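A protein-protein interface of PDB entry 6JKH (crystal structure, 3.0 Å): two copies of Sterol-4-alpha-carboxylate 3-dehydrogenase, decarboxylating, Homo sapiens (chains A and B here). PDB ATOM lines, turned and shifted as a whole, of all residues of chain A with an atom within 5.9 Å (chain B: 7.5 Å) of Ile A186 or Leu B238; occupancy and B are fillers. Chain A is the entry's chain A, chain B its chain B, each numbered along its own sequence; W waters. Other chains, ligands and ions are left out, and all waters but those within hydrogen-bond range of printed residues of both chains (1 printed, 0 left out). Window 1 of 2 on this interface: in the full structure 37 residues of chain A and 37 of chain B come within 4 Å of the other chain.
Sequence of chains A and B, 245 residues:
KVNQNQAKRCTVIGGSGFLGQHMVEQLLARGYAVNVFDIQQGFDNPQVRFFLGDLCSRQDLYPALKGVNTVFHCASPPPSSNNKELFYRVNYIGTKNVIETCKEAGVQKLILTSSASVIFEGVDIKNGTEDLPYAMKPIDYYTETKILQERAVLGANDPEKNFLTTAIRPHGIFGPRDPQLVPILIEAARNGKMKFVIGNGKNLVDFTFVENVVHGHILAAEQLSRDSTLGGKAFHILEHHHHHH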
ATOM      1  N   ILE A 119       8.855  12.615  17.738  1.00  0.00           N
ATOM      2  CA  ILE A 119       9.166  11.161  17.824  1.00  0.00           C
ATOM      3  C   ILE A 119       7.957  10.293  17.427  1.00  0.00           C
ATOM      4  O   ILE A 119       8.166   9.078  17.325  1.00  0.00           O
ATOM      5  CB  ILE A 119       9.711  10.778  19.208  1.00  0.00           C
ATOM      6  CG1 ILE A 119      10.569   9.511  19.115  1.00  0.00           C
ATOM      7  CG2 ILE A 119       8.574  10.639  20.204  1.00  0.00           C
ATOM      8  CD1 ILE A 119      11.331   9.182  20.371  1.00  0.00           C
ATOM      9  N   PRO A 183       6.740  10.821  25.520  1.00  0.00           N
ATOM     10  CA  PRO A 183       7.629   9.676  25.682  1.00  0.00           C
ATOM     11  C   PRO A 183       8.342   9.788  27.032  1.00  0.00           C
ATOM     12  O   PRO A 183       8.982  10.799  27.251  1.00  0.00           O
ATOM     13  CB  PRO A 183       8.608   9.808  24.511  1.00  0.00           C
ATOM     14  CG  PRO A 183       8.612  11.297  24.193  1.00  0.00           C
ATOM     15  CD  PRO A 183       7.207  11.769  24.497  1.00  0.00           C
ATOM     16  N   ILE A 184       8.157   8.799  27.906  1.00  0.00           N
ATOM     17  CA  ILE A 184       8.842   8.735  29.223  1.00  0.00           C
ATOM     18  C   ILE A 184      10.200   8.075  29.001  1.00  0.00           C
ATOM     19  O   ILE A 184      11.212   8.541  29.551  1.00  0.00           O
ATOM     20  CB  ILE A 184       7.991   7.960  30.244  1.00  0.00           C
ATOM     21  CG1 ILE A 184       6.750   8.750  30.655  1.00  0.00           C
ATOM     22  CG2 ILE A 184       8.826   7.581  31.459  1.00  0.00           C
ATOM     23  CD1 ILE A 184       7.051   9.952  31.545  1.00  0.00           C
ATOM     24  N   LEU A 185      10.210   6.997  28.228  1.00  0.00           N
ATOM     25  CA  LEU A 185      11.432   6.199  27.987  1.00  0.00           C
ATOM     26  C   LEU A 185      11.769   6.230  26.500  1.00  0.00           C
ATOM     27  O   LEU A 185      10.818   6.278  25.678  1.00  0.00           O
ATOM     28  CB  LEU A 185      11.181   4.770  28.453  1.00  0.00           C
ATOM     29  CG  LEU A 185      10.739   4.652  29.900  1.00  0.00           C
ATOM     30  CD1 LEU A 185      10.301   3.239  30.190  1.00  0.00           C
ATOM     31  CD2 LEU A 185      11.862   5.068  30.827  1.00  0.00           C
ATOM     32  N   ILE A 186      13.072   6.191  26.200  1.00  0.00           N
ATOM     33  CA  ILE A 186      13.639   6.159  24.822  1.00  0.00           C
ATOM     34  C   ILE A 186      14.655   5.028  24.739  1.00  0.00           C
ATOM     35  O   ILE A 186      15.480   4.918  25.652  1.00  0.00           O
ATOM     36  CB  ILE A 186      14.271   7.502  24.422  1.00  0.00           C
ATOM     37  CG1 ILE A 186      14.837   7.444  23.002  1.00  0.00           C
ATOM     38  CG2 ILE A 186      15.325   7.943  25.418  1.00  0.00           C
ATOM     39  CD1 ILE A 186      13.781   7.242  21.935  1.00  0.00           C
ATOM     40  N   GLU A 187      14.593   4.234  23.672  1.00  0.00           N
ATOM     41  CA  GLU A 187      15.481   3.062  23.497  1.00  0.00           C
ATOM     42  C   GLU A 187      16.891   3.588  23.280  1.00  0.00           C
ATOM     43  O   GLU A 187      17.067   4.681  22.763  1.00  0.00           O
ATOM     44  CB  GLU A 187      15.052   2.176  22.332  1.00  0.00           C
ATOM     45  CG  GLU A 187      15.498   0.725  22.469  1.00  0.00           C
ATOM     46  CD  GLU A 187      15.710  -0.046  21.164  1.00  0.00           C
ATOM     47  OE1 GLU A 187      14.798  -0.052  20.294  1.00  0.00           O
ATOM     48  OE2 GLU A 187      16.798  -0.649  21.010  1.00  0.00           O
ATOM     49  N   ALA A 188      17.862   2.817  23.709  1.00  0.00           N
ATOM     50  CA  ALA A 188      19.289   3.137  23.570  1.00  0.00           C
ATOM     51  C   ALA A 188      19.965   1.981  22.828  1.00  0.00           C
ATOM     52  O   ALA A 188      19.931   0.838  23.357  1.00  0.00           O
ATOM     53  CB  ALA A 188      19.869   3.374  24.944  1.00  0.00           C
ATOM     54  N   HIS A 236      17.068  14.329  22.126  1.00  0.00           N
ATOM     55  CA  HIS A 236      16.085  14.551  23.211  1.00  0.00           C
ATOM     56  C   HIS A 236      16.863  14.928  24.474  1.00  0.00           C
ATOM     57  O   HIS A 236      18.042  14.570  24.544  1.00  0.00           O
ATOM     58  CB  HIS A 236      15.265  13.285  23.409  1.00  0.00           C
ATOM     59  CG  HIS A 236      14.166  13.075  22.425  1.00  0.00           C
ATOM     60  ND1 HIS A 236      12.849  13.367  22.726  1.00  0.00           N
ATOM     61  CD2 HIS A 236      14.163  12.536  21.188  1.00  0.00           C
ATOM     62  CE1 HIS A 236      12.083  13.034  21.704  1.00  0.00           C
ATOM     63  NE2 HIS A 236      12.863  12.526  20.746  1.00  0.00           N
ATOM     64  N   ILE A 237      16.231  15.602  25.433  1.00  0.00           N
ATOM     65  CA  ILE A 237      16.868  15.992  26.726  1.00  0.00           C
ATOM     66  C   ILE A 237      16.491  14.957  27.800  1.00  0.00           C
ATOM     67  O   ILE A 237      15.675  14.063  27.503  1.00  0.00           O
ATOM     68  CB  ILE A 237      16.460  17.431  27.099  1.00  0.00           C
ATOM     69  CG1 ILE A 237      16.262  18.293  25.846  1.00  0.00           C
ATOM     70  CG2 ILE A 237      17.458  18.060  28.063  1.00  0.00           C
ATOM     71  CD1 ILE A 237      16.013  19.765  26.130  1.00  0.00           C
ATOM     72  N   LEU A 238      17.077  15.053  29.000  1.00  0.00           N
ATOM     73  CA  LEU A 238      16.885  14.079  30.109  1.00  0.00           C
ATOM     74  C   LEU A 238      16.446  14.778  31.406  1.00  0.00           C
ATOM     75  O   LEU A 238      16.558  16.023  31.475  1.00  0.00           O
ATOM     76  CB  LEU A 238      18.223  13.378  30.323  1.00  0.00           C
ATOM     77  CG  LEU A 238      18.809  12.720  29.083  1.00  0.00           C
ATOM     78  CD1 LEU A 238      20.249  12.311  29.332  1.00  0.00           C
ATOM     79  CD2 LEU A 238      17.972  11.520  28.667  1.00  0.00           C
ATOM     80  N   GLU A 239      16.008  13.985  32.402  1.00  0.00           N
ATOM     81  CA  GLU A 239      15.726  14.379  33.823  1.00  0.00           C
ATOM     82  C   GLU A 239      14.481  15.279  33.905  1.00  0.00           C
ATOM     83  O   GLU A 239      14.227  16.000  34.892  1.00  0.00           O
ATOM     84  CB  GLU A 239      16.916  15.093  34.485  1.00  0.00           C
ATOM     85  CG  GLU A 239      18.171  14.249  34.668  1.00  0.00           C
ATOM     86  CD  GLU A 239      19.134  14.161  33.489  1.00  0.00           C
ATOM     87  OE1 GLU A 239      18.842  14.723  32.414  1.00  0.00           O
ATOM     88  OE2 GLU A 239      20.194  13.526  33.657  1.00  0.00           O
ATOM     89  N   ALA B 167      16.131  -3.238  30.797  1.00  0.00           N
ATOM     90  CA  ALA B 167      16.933  -2.416  31.725  1.00  0.00           C
ATOM     91  C   ALA B 167      16.536  -0.960  31.516  1.00  0.00           C
ATOM     92  O   ALA B 167      16.315  -0.585  30.350  1.00  0.00           O
ATOM     93  CB  ALA B 167      18.404  -2.645  31.484  1.00  0.00           C
ATOM     94  N   ARG B 169      17.896   2.952  32.635  1.00  0.00           N
ATOM     95  CA  ARG B 169      19.169   3.611  33.015  1.00  0.00           C
ATOM     96  C   ARG B 169      18.859   4.978  33.595  1.00  0.00           C
ATOM     97  O   ARG B 169      18.917   5.979  32.887  1.00  0.00           O
ATOM     98  CB  ARG B 169      20.055   3.812  31.784  1.00  0.00           C
ATOM     99  CG  ARG B 169      20.557   2.544  31.111  1.00  0.00           C
ATOM    100  CD  ARG B 169      21.051   2.874  29.707  1.00  0.00           C
ATOM    101  NE  ARG B 169      21.738   1.770  29.035  1.00  0.00           N
ATOM    102  CZ  ARG B 169      22.395   1.859  27.878  1.00  0.00           C
ATOM    103  NH1 ARG B 169      22.474   3.012  27.243  1.00  0.00           N
ATOM    104  NH2 ARG B 169      22.979   0.793  27.358  1.00  0.00           N
ATOM    105  N   ILE B 184      23.717  14.999  28.711  1.00  0.00           N
ATOM    106  CA  ILE B 184      22.568  15.936  28.642  1.00  0.00           C
ATOM    107  C   ILE B 184      21.588  15.454  27.575  1.00  0.00           C
ATOM    108  O   ILE B 184      20.365  15.388  27.876  1.00  0.00           O
ATOM    109  CB  ILE B 184      23.068  17.359  28.344  1.00  0.00           C
ATOM    110  CG1 ILE B 184      24.201  17.765  29.284  1.00  0.00           C
ATOM    111  CG2 ILE B 184      21.922  18.357  28.395  1.00  0.00           C
ATOM    112  CD1 ILE B 184      23.868  17.597  30.749  1.00  0.00           C
ATOM    113  N   ILE B 186      20.666  12.936  23.902  1.00  0.00           N
ATOM    114  CA  ILE B 186      20.761  11.538  23.412  1.00  0.00           C
ATOM    115  C   ILE B 186      20.103  11.478  22.034  1.00  0.00           C
ATOM    116  O   ILE B 186      18.982  11.984  21.894  1.00  0.00           O
ATOM    117  CB  ILE B 186      20.105  10.580  24.427  1.00  0.00           C
ATOM    118  CG1 ILE B 186      19.955   9.156  23.879  1.00  0.00           C
ATOM    119  CG2 ILE B 186      18.768  11.134  24.899  1.00  0.00           C
ATOM    120  CD1 ILE B 186      19.790   8.091  24.951  1.00  0.00           C
ATOM    121  N   GLU B 187      20.784  10.885  21.059  1.00  0.00           N
ATOM    122  CA  GLU B 187      20.267  10.767  19.677  1.00  0.00           C
ATOM    123  C   GLU B 187      18.994   9.921  19.693  1.00  0.00           C
ATOM    124  O   GLU B 187      18.992   8.890  20.374  1.00  0.00           O
ATOM    125  CB  GLU B 187      21.309  10.130  18.768  1.00  0.00           C
ATOM    126  CG  GLU B 187      20.751   9.758  17.417  1.00  0.00           C
ATOM    127  CD  GLU B 187      21.735   9.043  16.510  1.00  0.00           C
ATOM    128  OE1 GLU B 187      22.946   9.016  16.842  1.00  0.00           O
ATOM    129  OE2 GLU B 187      21.284   8.512  15.470  1.00  0.00           O
ATOM    130  N   ALA B 188      17.957  10.352  18.974  1.00  0.00           N
ATOM    131  CA  ALA B 188      16.761   9.541  18.645  1.00  0.00           C
ATOM    132  C   ALA B 188      16.797   9.183  17.157  1.00  0.00           C
ATOM    133  O   ALA B 188      16.741  10.126  16.349  1.00  0.00           O
ATOM    134  CB  ALA B 188      15.516  10.310  18.992  1.00  0.00           C
ATOM    135  N   ALA B 189      16.881   7.891  16.809  1.00  0.00           N
ATOM    136  CA  ALA B 189      17.015   7.392  15.416  1.00  0.00           C
ATOM    137  C   ALA B 189      15.686   7.594  14.682  1.00  0.00           C
ATOM    138  O   ALA B 189      14.644   7.288  15.285  1.00  0.00           O
ATOM    139  CB  ALA B 189      17.419   5.941  15.410  1.00  0.00           C
ATOM    140  N   MET B 194      14.471   2.449  16.798  1.00  0.00           N
ATOM    141  CA  MET B 194      14.300   2.595  18.258  1.00  0.00           C
ATOM    142  C   MET B 194      12.825   2.569  18.651  1.00  0.00           C
ATOM    143  O   MET B 194      11.977   2.877  17.810  1.00  0.00           O
ATOM    144  CB  MET B 194      14.992   3.857  18.764  1.00  0.00           C
ATOM    145  CG  MET B 194      14.083   4.763  19.498  1.00  0.00           C
ATOM    146  SD  MET B 194      13.947   6.250  18.546  1.00  0.00           S
ATOM    147  CE  MET B 194      12.368   5.967  17.749  1.00  0.00           C
ATOM    148  N   LYS B 195      12.581   2.176  19.903  1.00  0.00           N
ATOM    149  CA  LYS B 195      11.254   2.053  20.547  1.00  0.00           C
ATOM    150  C   LYS B 195      11.209   2.990  21.745  1.00  0.00           C
ATOM    151  O   LYS B 195      12.226   3.188  22.372  1.00  0.00           O
ATOM    152  CB  LYS B 195      11.070   0.643  21.097  1.00  0.00           C
ATOM    153  CG  LYS B 195      11.121  -0.467  20.068  1.00  0.00           C
ATOM    154  CD  LYS B 195       9.999  -0.381  19.073  1.00  0.00           C
ATOM    155  CE  LYS B 195      10.005  -1.525  18.089  1.00  0.00           C
ATOM    156  NZ  LYS B 195       8.904  -1.396  17.113  1.00  0.00           N
ATOM    157  N   PHE B 196      10.042   3.539  22.023  1.00  0.00           N
ATOM    158  CA  PHE B 196       9.847   4.452  23.164  1.00  0.00           C
ATOM    159  C   PHE B 196       8.610   4.000  23.930  1.00  0.00           C
ATOM    160  O   PHE B 196       7.919   3.080  23.511  1.00  0.00           O
ATOM    161  CB  PHE B 196       9.697   5.889  22.680  1.00  0.00           C
ATOM    162  CG  PHE B 196       8.755   6.069  21.521  1.00  0.00           C
ATOM    163  CD1 PHE B 196       9.107   5.649  20.253  1.00  0.00           C
ATOM    164  CD2 PHE B 196       7.524   6.665  21.697  1.00  0.00           C
ATOM    165  CE1 PHE B 196       8.248   5.815  19.183  1.00  0.00           C
ATOM    166  CE2 PHE B 196       6.666   6.830  20.628  1.00  0.00           C
ATOM    167  CZ  PHE B 196       7.031   6.408  19.377  1.00  0.00           C
ATOM    168  N   VAL B 197       8.389   4.612  25.076  1.00  0.00           N
ATOM    169  CA  VAL B 197       7.242   4.266  25.943  1.00  0.00           C
ATOM    170  C   VAL B 197       6.533   5.569  26.220  1.00  0.00           C
ATOM    171  O   VAL B 197       7.213   6.514  26.672  1.00  0.00           O
ATOM    172  CB  VAL B 197       7.690   3.579  27.237  1.00  0.00           C
ATOM    173  CG1 VAL B 197       6.534   3.376  28.201  1.00  0.00           C
ATOM    174  CG2 VAL B 197       8.385   2.263  26.937  1.00  0.00           C
ATOM    175  N   PHE B 209      11.615  13.739  40.887  1.00  0.00           N
ATOM    176  CA  PHE B 209      12.546  13.079  39.941  1.00  0.00           C
ATOM    177  C   PHE B 209      12.439  11.573  40.154  1.00  0.00           C
ATOM    178  O   PHE B 209      12.329  10.810  39.175  1.00  0.00           O
ATOM    179  CB  PHE B 209      13.983  13.575  40.133  1.00  0.00           C
ATOM    180  CG  PHE B 209      15.015  12.856  39.296  1.00  0.00           C
ATOM    181  CD1 PHE B 209      14.876  12.767  37.920  1.00  0.00           C
ATOM    182  CD2 PHE B 209      16.126  12.254  39.871  1.00  0.00           C
ATOM    183  CE1 PHE B 209      15.817  12.096  37.148  1.00  0.00           C
ATOM    184  CE2 PHE B 209      17.065  11.579  39.095  1.00  0.00           C
ATOM    185  CZ  PHE B 209      16.912  11.502  37.733  1.00  0.00           C
ATOM    186  N   ASN B 212       9.218   9.824  39.072  1.00  0.00           N
ATOM    187  CA  ASN B 212       9.192   9.714  37.588  1.00  0.00           C
ATOM    188  C   ASN B 212      10.034   8.511  37.147  1.00  0.00           C
ATOM    189  O   ASN B 212       9.549   7.711  36.339  1.00  0.00           O
ATOM    190  CB  ASN B 212       9.623  11.016  36.900  1.00  0.00           C
ATOM    191  CG  ASN B 212       8.452  11.773  36.298  1.00  0.00           C
ATOM    192  OD1 ASN B 212       7.893  11.369  35.276  1.00  0.00           O
ATOM    193  ND2 ASN B 212       8.059  12.870  36.925  1.00  0.00           N
ATOM    194  N   ALA B 234      17.672  -1.681  26.398  1.00  0.00           N
ATOM    195  CA  ALA B 234      17.908  -0.737  27.509  1.00  0.00           C
ATOM    196  C   ALA B 234      17.293   0.602  27.114  1.00  0.00           C
ATOM    197  O   ALA B 234      17.274   0.881  25.922  1.00  0.00           O
ATOM    198  CB  ALA B 234      19.387  -0.587  27.767  1.00  0.00           C
ATOM    199  N   PHE B 235      16.816   1.371  28.092  1.00  0.00           N
ATOM    200  CA  PHE B 235      15.994   2.591  27.914  1.00  0.00           C
ATOM    201  C   PHE B 235      16.534   3.708  28.794  1.00  0.00           C
ATOM    202  O   PHE B 235      17.115   3.427  29.876  1.00  0.00           O
ATOM    203  CB  PHE B 235      14.535   2.337  28.280  1.00  0.00           C
ATOM    204  CG  PHE B 235      13.869   1.340  27.371  1.00  0.00           C
ATOM    205  CD1 PHE B 235      13.251   1.753  26.201  1.00  0.00           C
ATOM    206  CD2 PHE B 235      13.899  -0.017  27.652  1.00  0.00           C
ATOM    207  CE1 PHE B 235      12.656   0.830  25.350  1.00  0.00           C
ATOM    208  CE2 PHE B 235      13.312  -0.939  26.794  1.00  0.00           C
ATOM    209  CZ  PHE B 235      12.682  -0.514  25.649  1.00  0.00           C
ATOM    210  N   HIS B 236      16.313   4.926  28.320  1.00  0.00           N
ATOM    211  CA  HIS B 236      16.698   6.170  29.009  1.00  0.00           C
ATOM    212  C   HIS B 236      15.429   6.895  29.415  1.00  0.00           C
ATOM    213  O   HIS B 236      14.416   6.695  28.785  1.00  0.00           O
ATOM    214  CB  HIS B 236      17.557   7.014  28.092  1.00  0.00           C
ATOM    215  CG  HIS B 236      18.998   6.831  28.364  1.00  0.00           C
ATOM    216  ND1 HIS B 236      19.817   6.166  27.515  1.00  0.00           N
ATOM    217  CD2 HIS B 236      19.753   7.197  29.407  1.00  0.00           C
ATOM    218  CE1 HIS B 236      21.022   6.133  28.017  1.00  0.00           C
ATOM    219  NE2 HIS B 236      21.005   6.753  29.165  1.00  0.00           N
ATOM    220  N   ILE B 237      15.517   7.709  30.454  1.00  0.00           N
ATOM    221  CA  ILE B 237      14.353   8.475  30.985  1.00  0.00           C
ATOM    222  C   ILE B 237      14.415   9.917  30.482  1.00  0.00           C
ATOM    223  O   ILE B 237      15.471  10.550  30.594  1.00  0.00           O
ATOM    224  CB  ILE B 237      14.331   8.400  32.510  1.00  0.00           C
ATOM    225  CG1 ILE B 237      14.419   6.944  32.968  1.00  0.00           C
ATOM    226  CG2 ILE B 237      13.097   9.100  33.041  1.00  0.00           C
ATOM    227  CD1 ILE B 237      14.877   6.780  34.411  1.00  0.00           C
ATOM    228  N   LEU B 238      13.304  10.406  29.946  1.00  0.00           N
ATOM    229  CA  LEU B 238      13.231  11.729  29.288  1.00  0.00           C
ATOM    230  C   LEU B 238      12.599  12.761  30.219  1.00  0.00           C
ATOM    231  O   LEU B 238      12.152  12.393  31.310  1.00  0.00           O
ATOM    232  CB  LEU B 238      12.400  11.597  28.011  1.00  0.00           C
ATOM    233  CG  LEU B 238      13.002  10.742  26.903  1.00  0.00           C
ATOM    234  CD1 LEU B 238      12.135  10.811  25.656  1.00  0.00           C
ATOM    235  CD2 LEU B 238      14.419  11.170  26.573  1.00  0.00           C
ATOM    236  N   GLU B 239      12.547  14.002  29.733  1.00  0.00           N
ATOM    237  CA  GLU B 239      11.953  15.197  30.376  1.00  0.00           C
ATOM    238  C   GLU B 239      10.483  14.961  30.727  1.00  0.00           C
ATOM    239  O   GLU B 239       9.864  15.844  31.322  1.00  0.00           O
ATOM    240  CB  GLU B 239      12.077  16.387  29.423  1.00  0.00           C
ATOM    241  CG  GLU B 239      11.746  17.714  30.076  1.00  0.00           C
ATOM    242  CD  GLU B 239      12.223  17.867  31.518  1.00  0.00           C
ATOM    243  OE1 GLU B 239      13.331  17.371  31.845  1.00  0.00           O
ATOM    244  OE2 GLU B 239      11.470  18.459  32.325  1.00  0.00           O
HETATM  245  O   HOH W   1      19.080  -1.568  23.544  1.00  0.00           O
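Water W1 lies within hydrogen-bond range of the backbone carbonyl oxygen (O) of Ala A188 (2.6 Å) and the backbone NH (N) of Ala B234 (3.2 Å).
Ile A184 touches Leu B238, and with the chains exchanged Leu A238 touches Ile B184.
Ile A186 touches His B236, and with the chains exchanged His A236 touches Ile B186.
His A236 touches Leu B238, but with the chains exchanged Leu A238 does not touch His B236 (4.6 Å).
Leu A238 touches Glu B239, but with the chains exchanged Glu A239 does not touch Leu B238 (4.2 Å).
Positions printed for both chains: 184, 186, 187, 188, 236, 237, 238 and 239.
Hydrophobic or aromatic side chains of chain B that line the printed part of chain A: Ile B186, Ala B188, Met B194, Phe B196, Val B197, Phe B235, His B236, Ile B237 and Leu B238.
Printed residues of chain B within 4 Å of Ile A119: Phe B196.
Printed residues of chain A within 4 Å of Ala B234: Glu A187 and Ala A188.
Ala B167 touches none of the printed residues of chain A.
Asn B212 touches none of the printed residues of chain A.
The nearest printed residue of chain A that does not touch Lys B195 is Leu A185 (4.7 Å).
The backbone NH (N) of Ile A184 sits at hydrogen-bond distance from the backbone carbonyl oxygen (O) of Val B197 (2.8 Å).
N of Leu B238 sits at hydrogen-bond distance from O of Ile A184 (2.8 Å).
The backbone carbonyl oxygen (O) of Leu A185 is in hydrogen-bond range of the backbone NH (N) of Val B197 (3.0 Å).
O of Ile A186 is in hydrogen-bond range of N of His B236, at 2.8 Å.
The backbone NH (N) of Glu A187 is in hydrogen-bond range of the backbone carbonyl oxygen (O) of Lys B195.
O of Ala B234 is in hydrogen-bond range of N of Ala A188 (3.0 Å).
O of Ile B186 sits at hydrogen-bond distance from N of His A236.
N of Leu A238 sits close to O of Ile B184.
The side-chain carboxylate of Glu B239 sits close to the backbone carbonyl oxygen of Glu A239 (3.5 Å).
The backbone NH (N) of Phe B235 lies within hydrogen-bond range of the backbone carbonyl oxygen (O) of Ala B167 (3.0 Å).
O of Phe B235 sits at hydrogen-bond distance from N of Arg B169, 2.9 Å away.
N of Ala B189 lies within hydrogen-bond range of SD of Met B194, 3.8 Å away.
Pro A183 touches Val B197.
Ile A184 touches His B236.
CA of Ile B237 touches O of Ile A184, 3.5 Å away.
CA of Leu A185 touches O of His B236 (3.1 Å).
Ala B234 touches Glu A187 (O to CA, 3.7 Å).
His A236 touches Leu B238 (CB to CD2, 3.9 Å).
O of Ile B184 touches CA of Ile A237, 3.7 Å away.
Leu B238 touches Ile A237 (CD2 to O, 3.3 Å).
Glu B239 touches Ile A237.
O of Leu A238 touches OE1 of Glu B239, at 3.5 Å.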
